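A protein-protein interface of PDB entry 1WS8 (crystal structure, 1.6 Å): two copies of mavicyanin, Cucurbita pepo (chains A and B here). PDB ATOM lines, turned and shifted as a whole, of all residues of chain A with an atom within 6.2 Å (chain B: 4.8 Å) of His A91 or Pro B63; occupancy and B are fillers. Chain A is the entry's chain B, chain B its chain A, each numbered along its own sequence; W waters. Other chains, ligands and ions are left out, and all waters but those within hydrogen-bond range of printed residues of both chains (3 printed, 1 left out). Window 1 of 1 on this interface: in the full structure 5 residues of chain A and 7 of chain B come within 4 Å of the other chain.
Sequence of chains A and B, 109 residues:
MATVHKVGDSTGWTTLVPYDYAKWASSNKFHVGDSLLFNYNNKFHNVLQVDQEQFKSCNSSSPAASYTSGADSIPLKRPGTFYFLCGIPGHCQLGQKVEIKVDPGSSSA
A ring nitrogen (NE2) of His A91 sits at hydrogen-bond distance from the backbone carbonyl oxygen (O) of Pro B63, at 2.8 Å.
The backbone carbonyl oxygen of Ala B65 sits at hydrogen-bond distance from the backbone NH of Gln B49, 2.9 Å away. SG of Cys A92 forms a disulfide with SG of Cys A58, 2.0 Å away. The backbone carbonyl oxygen (O) of Gln B49 is in hydrogen-bond range of the backbone NH (N) of Ala B64, 2.8 Å away.
CB of Phe A44 touches O of Ala B64, at 3.4 Å. Ala B65 touches Phe A44 (CB to CE1, 3.6 Å). O of Pro A89 touches O of Ser B61 (3.7 Å). Pro A89 touches Ser B62 (O to OG, 3.5 Å). Gly A90 touches Ser B62 (CA to OG, 3.1 Å).
Of the printed residues of chain B, Pro A89 touches Ser B61 (3.7 Å) and Ser B62 (3.5 Å). His A91 touches just one residue of chain B: Pro B63 (2.8 Å). Gln B49 touches none of the printed residues of chain A. Pro B63 touches one residue of chain A. Of the printed residues of chain A, Ala B65 touches Phe A44. The nearest printed residue of chain B that does not touch Phe A44 is Pro B63 (5.4 Å).
Hydrophobic or aromatic side chains of chain A that line the printed part of chain B: Phe A44 and His A91. Of the 9 printed residues of chain B, 5 touch a printed residue of chain A. Printed residues of chain B that touch a printed residue of chain A: Ser B61, Ser B62, Pro B63, Ala B64 and Ala B65. Hydrophobic or aromatic side chains of chain B within 4 Å of the printed part of chain A: Ala B65.
No position is printed for both chains.
Water W1 lies within hydrogen-bond range of the side-chain hydroxyl of Thr A15, the backbone carbonyl oxygen of Ser B62 and the backbone NH of Ala B64. Water W2 lies within hydrogen-bond range of the backbone carbonyl oxygen (O) of Gly A90 (2.9 Å) and the side-chain hydroxyl (OG) of Ser B62 (3.1 Å). Water W3 lies within hydrogen-bond range of the backbone carbonyl oxygen of Ser B61 (3.0 Å), the side-chain hydroxyl of Ser B62 (3.3 Å) and the backbone NH of Gly A90 (3.5 Å).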
ATOM      1  N   THR A  15     -28.458 -13.214 -12.050  1.00  0.00           N
ATOM      2  CA  THR A  15     -28.749 -11.817 -12.367  1.00  0.00           C
ATOM      3  C   THR A  15     -27.567 -11.224 -13.138  1.00  0.00           C
ATOM      4  O   THR A  15     -27.579 -10.045 -13.485  1.00  0.00           O
ATOM      5  CB  THR A  15     -28.954 -10.948 -11.100  1.00  0.00           C
ATOM      6  OG1 THR A  15     -27.823 -11.101 -10.233  1.00  0.00           O
ATOM      7  CG2 THR A  15     -30.222 -11.350 -10.367  1.00  0.00           C
ATOM      8  N   PHE A  44     -24.563 -16.159  -3.322  1.00  0.00           N
ATOM      9  CA  PHE A  44     -25.102 -14.913  -3.857  1.00  0.00           C
ATOM     10  C   PHE A  44     -26.573 -14.875  -4.252  1.00  0.00           C
ATOM     11  O   PHE A  44     -27.064 -13.826  -4.666  1.00  0.00           O
ATOM     12  CB  PHE A  44     -24.258 -14.501  -5.064  1.00  0.00           C
ATOM     13  CG  PHE A  44     -22.781 -14.492  -4.787  1.00  0.00           C
ATOM     14  CD1 PHE A  44     -21.894 -15.114  -5.657  1.00  0.00           C
ATOM     15  CD2 PHE A  44     -22.279 -13.867  -3.651  1.00  0.00           C
ATOM     16  CE1 PHE A  44     -20.523 -15.116  -5.398  1.00  0.00           C
ATOM     17  CE2 PHE A  44     -20.913 -13.863  -3.383  1.00  0.00           C
ATOM     18  CZ  PHE A  44     -20.035 -14.489  -4.256  1.00  0.00           C
ATOM     19  N   HIS A  45     -27.268 -16.004  -4.138  1.00  0.00           N
ATOM     20  CA  HIS A  45     -28.688 -16.075  -4.488  1.00  0.00           C
ATOM     21  C   HIS A  45     -29.379 -17.109  -3.611  1.00  0.00           C
ATOM     22  O   HIS A  45     -28.731 -17.897  -2.919  1.00  0.00           O
ATOM     23  CB  HIS A  45     -28.883 -16.536  -5.945  1.00  0.00           C
ATOM     24  CG  HIS A  45     -28.230 -15.661  -6.969  1.00  0.00           C
ATOM     25  ND1 HIS A  45     -28.753 -14.449  -7.359  1.00  0.00           N
ATOM     26  CD2 HIS A  45     -27.100 -15.836  -7.695  1.00  0.00           C
ATOM     27  CE1 HIS A  45     -27.975 -13.914  -8.283  1.00  0.00           C
ATOM     28  NE2 HIS A  45     -26.965 -14.736  -8.504  1.00  0.00           N
ATOM     29  N   CYS A  58     -42.333  -8.008  -5.095  1.00  0.00           N
ATOM     30  CA  CYS A  58     -40.982  -8.454  -4.781  1.00  0.00           C
ATOM     31  C   CYS A  58     -40.695  -8.404  -3.284  1.00  0.00           C
ATOM     32  O   CYS A  58     -39.607  -8.008  -2.858  1.00  0.00           O
ATOM     33  CB  CYS A  58     -39.957  -7.602  -5.527  1.00  0.00           C
ATOM     34  SG  CYS A  58     -39.599  -8.165  -7.217  1.00  0.00           S
ATOM     35  N   CYS A  86     -35.848 -14.533  -5.935  1.00  0.00           N
ATOM     36  CA  CYS A  86     -34.603 -14.516  -5.187  1.00  0.00           C
ATOM     37  C   CYS A  86     -34.771 -13.383  -4.185  1.00  0.00           C
ATOM     38  O   CYS A  86     -35.128 -12.267  -4.564  1.00  0.00           O
ATOM     39  CB  CYS A  86     -33.415 -14.222  -6.097  1.00  0.00           C
ATOM     40  SG  CYS A  86     -31.862 -14.044  -5.176  1.00  0.00           S
ATOM     41  N   GLY A  87     -34.516 -13.681  -2.913  1.00  0.00           N
ATOM     42  CA  GLY A  87     -34.673 -12.687  -1.867  1.00  0.00           C
ATOM     43  C   GLY A  87     -33.494 -11.769  -1.611  1.00  0.00           C
ATOM     44  O   GLY A  87     -33.583 -10.885  -0.760  1.00  0.00           O
ATOM     45  N   ILE A  88     -32.389 -11.965  -2.324  1.00  0.00           N
ATOM     46  CA  ILE A  88     -31.226 -11.103  -2.135  1.00  0.00           C
ATOM     47  C   ILE A  88     -31.642  -9.702  -2.578  1.00  0.00           C
ATOM     48  O   ILE A  88     -32.254  -9.528  -3.633  1.00  0.00           O
ATOM     49  CB  ILE A  88     -30.022 -11.597  -2.969  1.00  0.00           C
ATOM     50  CG1 ILE A  88     -29.644 -13.016  -2.537  1.00  0.00           C
ATOM     51  CG2 ILE A  88     -28.834 -10.647  -2.812  1.00  0.00           C
ATOM     52  CD1 ILE A  88     -29.300 -13.158  -1.062  1.00  0.00           C
ATOM     53  N   PRO A  89     -31.328  -8.680  -1.766  1.00  0.00           N
ATOM     54  CA  PRO A  89     -31.684  -7.296  -2.085  1.00  0.00           C
ATOM     55  C   PRO A  89     -31.560  -6.893  -3.552  1.00  0.00           C
ATOM     56  O   PRO A  89     -30.486  -6.993  -4.145  1.00  0.00           O
ATOM     57  CB  PRO A  89     -30.754  -6.495  -1.180  1.00  0.00           C
ATOM     58  CG  PRO A  89     -30.720  -7.344   0.048  1.00  0.00           C
ATOM     59  CD  PRO A  89     -30.517  -8.734  -0.535  1.00  0.00           C
ATOM     60  N   GLY A  90     -32.681  -6.459  -4.124  1.00  0.00           N
ATOM     61  CA  GLY A  90     -32.706  -6.004  -5.502  1.00  0.00           C
ATOM     62  C   GLY A  90     -32.740  -7.026  -6.626  1.00  0.00           C
ATOM     63  O   GLY A  90     -33.048  -6.667  -7.762  1.00  0.00           O
ATOM     64  N   HIS A  91     -32.438  -8.288  -6.338  1.00  0.00           N
ATOM     65  CA  HIS A  91     -32.434  -9.296  -7.394  1.00  0.00           C
ATOM     66  C   HIS A  91     -33.800  -9.557  -8.010  1.00  0.00           C
ATOM     67  O   HIS A  91     -33.908  -9.782  -9.214  1.00  0.00           O
ATOM     68  CB  HIS A  91     -31.841 -10.612  -6.884  1.00  0.00           C
ATOM     69  CG  HIS A  91     -30.360 -10.561  -6.690  1.00  0.00           C
ATOM     70  ND1 HIS A  91     -29.589 -11.692  -6.530  1.00  0.00           N
ATOM     71  CD2 HIS A  91     -29.505  -9.511  -6.636  1.00  0.00           C
ATOM     72  CE1 HIS A  91     -28.323 -11.341  -6.388  1.00  0.00           C
ATOM     73  NE2 HIS A  91     -28.245 -10.025  -6.449  1.00  0.00           N
ATOM     74  N   CYS A  92     -34.838  -9.544  -7.183  1.00  0.00           N
ATOM     75  CA  CYS A  92     -36.191  -9.770  -7.674  1.00  0.00           C
ATOM     76  C   CYS A  92     -36.574  -8.633  -8.619  1.00  0.00           C
ATOM     77  O   CYS A  92     -37.196  -8.858  -9.658  1.00  0.00           O
ATOM     78  CB  CYS A  92     -37.163  -9.823  -6.500  1.00  0.00           C
ATOM     79  SG  CYS A  92     -38.922 -10.056  -6.925  1.00  0.00           S
ATOM     80  N   GLN A  93     -36.193  -7.413  -8.254  1.00  0.00           N
ATOM     81  CA  GLN A  93     -36.505  -6.246  -9.068  1.00  0.00           C
ATOM     82  C   GLN A  93     -35.781  -6.265 -10.414  1.00  0.00           C
ATOM     83  O   GLN A  93     -36.252  -5.674 -11.385  1.00  0.00           O
ATOM     84  CB  GLN A  93     -36.175  -4.962  -8.299  1.00  0.00           C
ATOM     85  CG  GLN A  93     -37.044  -4.753  -7.064  1.00  0.00           C
ATOM     86  CD  GLN A  93     -36.474  -5.390  -5.804  1.00  0.00           C
ATOM     87  OE1 GLN A  93     -35.998  -6.529  -5.818  1.00  0.00           O
ATOM     88  NE2 GLN A  93     -36.533  -4.655  -4.698  1.00  0.00           N
ATOM     89  N   LEU A  94     -34.639  -6.946 -10.472  1.00  0.00           N
ATOM     90  CA  LEU A  94     -33.879  -7.054 -11.712  1.00  0.00           C
ATOM     91  C   LEU A  94     -34.497  -8.124 -12.605  1.00  0.00           C
ATOM     92  O   LEU A  94     -34.048  -8.333 -13.733  1.00  0.00           O
ATOM     93  CB  LEU A  94     -32.420  -7.417 -11.423  1.00  0.00           C
ATOM     94  CG  LEU A  94     -31.552  -6.352 -10.753  1.00  0.00           C
ATOM     95  CD1 LEU A  94     -30.211  -6.958 -10.375  1.00  0.00           C
ATOM     96  CD2 LEU A  94     -31.359  -5.175 -11.700  1.00  0.00           C
ATOM     97  N   GLY A  95     -35.511  -8.815 -12.087  1.00  0.00           N
ATOM     98  CA  GLY A  95     -36.180  -9.840 -12.868  1.00  0.00           C
ATOM     99  C   GLY A  95     -35.960 -11.282 -12.453  1.00  0.00           C
ATOM    100  O   GLY A  95     -36.422 -12.194 -13.140  1.00  0.00           O
ATOM    101  N   GLN A  96     -35.264 -11.510 -11.343  1.00  0.00           N
ATOM    102  CA  GLN A  96     -35.024 -12.881 -10.906  1.00  0.00           C
ATOM    103  C   GLN A  96     -36.209 -13.394 -10.092  1.00  0.00           C
ATOM    104  O   GLN A  96     -36.171 -13.484  -8.862  1.00  0.00           O
ATOM    105  CB  GLN A  96     -33.722 -12.972 -10.101  1.00  0.00           C
ATOM    106  CG  GLN A  96     -33.268 -14.401  -9.854  1.00  0.00           C
ATOM    107  CD  GLN A  96     -31.933 -14.469  -9.137  1.00  0.00           C
ATOM    108  OE1 GLN A  96     -31.536 -13.517  -8.473  1.00  0.00           O
ATOM    109  NE2 GLN A  96     -31.244 -15.601  -9.256  1.00  0.00           N
ATOM    110  N   LYS A  97     -37.272 -13.728 -10.812  1.00  0.00           N
ATOM    111  CA  LYS A  97     -38.500 -14.227 -10.219  1.00  0.00           C
ATOM    112  C   LYS A  97     -39.176 -15.042 -11.313  1.00  0.00           C
ATOM    113  O   LYS A  97     -38.966 -14.784 -12.499  1.00  0.00           O
ATOM    114  CB  LYS A  97     -39.399 -13.058  -9.815  1.00  0.00           C
ATOM    115  CG  LYS A  97     -39.671 -12.100 -10.972  1.00  0.00           C
ATOM    116  CD  LYS A  97     -40.973 -11.334 -10.811  1.00  0.00           C
ATOM    117  CE  LYS A  97     -40.937 -10.351  -9.664  1.00  0.00           C
ATOM    118  NZ  LYS A  97     -42.166  -9.502  -9.660  1.00  0.00           N
ATOM    119  N   LEU B  48     -17.552  -5.519  -5.190  1.00  0.00           N
ATOM    120  CA  LEU B  48     -18.851  -5.997  -5.644  1.00  0.00           C
ATOM    121  C   LEU B  48     -18.822  -6.152  -7.149  1.00  0.00           C
ATOM    122  O   LEU B  48     -18.253  -5.319  -7.855  1.00  0.00           O
ATOM    123  CB  LEU B  48     -19.953  -5.001  -5.281  1.00  0.00           C
ATOM    124  CG  LEU B  48     -20.070  -4.590  -3.809  1.00  0.00           C
ATOM    125  CD1 LEU B  48     -21.251  -3.648  -3.660  1.00  0.00           C
ATOM    126  CD2 LEU B  48     -20.245  -5.811  -2.928  1.00  0.00           C
ATOM    127  N   GLN B  49     -19.420  -7.232  -7.640  1.00  0.00           N
ATOM    128  CA  GLN B  49     -19.493  -7.440  -9.079  1.00  0.00           C
ATOM    129  C   GLN B  49     -20.870  -6.931  -9.487  1.00  0.00           C
ATOM    130  O   GLN B  49     -21.873  -7.288  -8.874  1.00  0.00           O
ATOM    131  CB  GLN B  49     -19.354  -8.918  -9.438  1.00  0.00           C
ATOM    132  CG  GLN B  49     -19.434  -9.145 -10.946  1.00  0.00           C
ATOM    133  CD  GLN B  49     -19.233 -10.594 -11.333  1.00  0.00           C
ATOM    134  OE1 GLN B  49     -19.223 -11.481 -10.482  1.00  0.00           O
ATOM    135  NE2 GLN B  49     -19.083 -10.840 -12.628  1.00  0.00           N
ATOM    136  N   VAL B  50     -20.910  -6.090 -10.514  1.00  0.00           N
ATOM    137  CA  VAL B  50     -22.161  -5.492 -10.973  1.00  0.00           C
ATOM    138  C   VAL B  50     -22.250  -5.554 -12.491  1.00  0.00           C
ATOM    139  O   VAL B  50     -21.337  -6.052 -13.144  1.00  0.00           O
ATOM    140  CB  VAL B  50     -22.232  -4.010 -10.545  1.00  0.00           C
ATOM    141  CG1 VAL B  50     -22.245  -3.899  -9.018  1.00  0.00           C
ATOM    142  CG2 VAL B  50     -21.038  -3.250 -11.121  1.00  0.00           C
ATOM    143  N   SER B  60     -24.613   0.348  -6.144  1.00  0.00           N
ATOM    144  CA  SER B  60     -24.125  -0.823  -5.421  1.00  0.00           C
ATOM    145  C   SER B  60     -25.220  -1.496  -4.599  1.00  0.00           C
ATOM    146  O   SER B  60     -24.931  -2.289  -3.705  1.00  0.00           O
ATOM    147  CB  SER B  60     -22.978  -0.413  -4.495  1.00  0.00           C
ATOM    148  OG  SER B  60     -23.410   0.574  -3.571  1.00  0.00           O
ATOM    149  N   SER B  61     -26.473  -1.196  -4.917  1.00  0.00           N
ATOM    150  CA  SER B  61     -27.600  -1.746  -4.171  1.00  0.00           C
ATOM    151  C   SER B  61     -27.987  -3.187  -4.487  1.00  0.00           C
ATOM    152  O   SER B  61     -28.607  -3.851  -3.657  1.00  0.00           O
ATOM    153  CB  SER B  61     -28.832  -0.859  -4.362  1.00  0.00           C
ATOM    154  OG  SER B  61     -29.295  -0.922  -5.699  1.00  0.00           O
ATOM    155  N   SER B  62     -27.629  -3.675  -5.672  1.00  0.00           N
ATOM    156  CA  SER B  62     -27.995  -5.041  -6.051  1.00  0.00           C
ATOM    157  C   SER B  62     -26.879  -5.773  -6.783  1.00  0.00           C
ATOM    158  O   SER B  62     -27.003  -6.087  -7.966  1.00  0.00           O
ATOM    159  CB  SER B  62     -29.242  -5.007  -6.934  1.00  0.00           C
ATOM    160  OG  SER B  62     -30.267  -4.249  -6.321  1.00  0.00           O
ATOM    161  N   PRO B  63     -25.778  -6.074  -6.080  1.00  0.00           N
ATOM    162  CA  PRO B  63     -24.619  -6.770  -6.651  1.00  0.00           C
ATOM    163  C   PRO B  63     -24.891  -8.218  -7.046  1.00  0.00           C
ATOM    164  O   PRO B  63     -25.703  -8.896  -6.425  1.00  0.00           O
ATOM    165  CB  PRO B  63     -23.577  -6.692  -5.531  1.00  0.00           C
ATOM    166  CG  PRO B  63     -24.047  -5.559  -4.668  1.00  0.00           C
ATOM    167  CD  PRO B  63     -25.528  -5.721  -4.673  1.00  0.00           C
ATOM    168  N   ALA B  64     -24.194  -8.688  -8.074  1.00  0.00           N
ATOM    169  CA  ALA B  64     -24.335 -10.068  -8.528  1.00  0.00           C
ATOM    170  C   ALA B  64     -23.462 -10.953  -7.636  1.00  0.00           C
ATOM    171  O   ALA B  64     -23.694 -12.157  -7.502  1.00  0.00           O
ATOM    172  CB  ALA B  64     -23.893 -10.183  -9.980  1.00  0.00           C
ATOM    173  N   ALA B  65     -22.446 -10.345  -7.031  1.00  0.00           N
ATOM    174  CA  ALA B  65     -21.536 -11.063  -6.144  1.00  0.00           C
ATOM    175  C   ALA B  65     -20.811 -10.064  -5.252  1.00  0.00           C
ATOM    176  O   ALA B  65     -20.631  -8.903  -5.620  1.00  0.00           O
ATOM    177  CB  ALA B  65     -20.523 -11.872  -6.955  1.00  0.00           C
HETATM  178  O   HOH W   1     -27.206  -8.492  -9.618  1.00  0.00           O
HETATM  179  O   HOH W   2     -32.630  -3.837  -8.346  1.00  0.00           O
HETATM  180  O   HOH W   3     -31.547  -3.208  -3.496  1.00  0.00           O
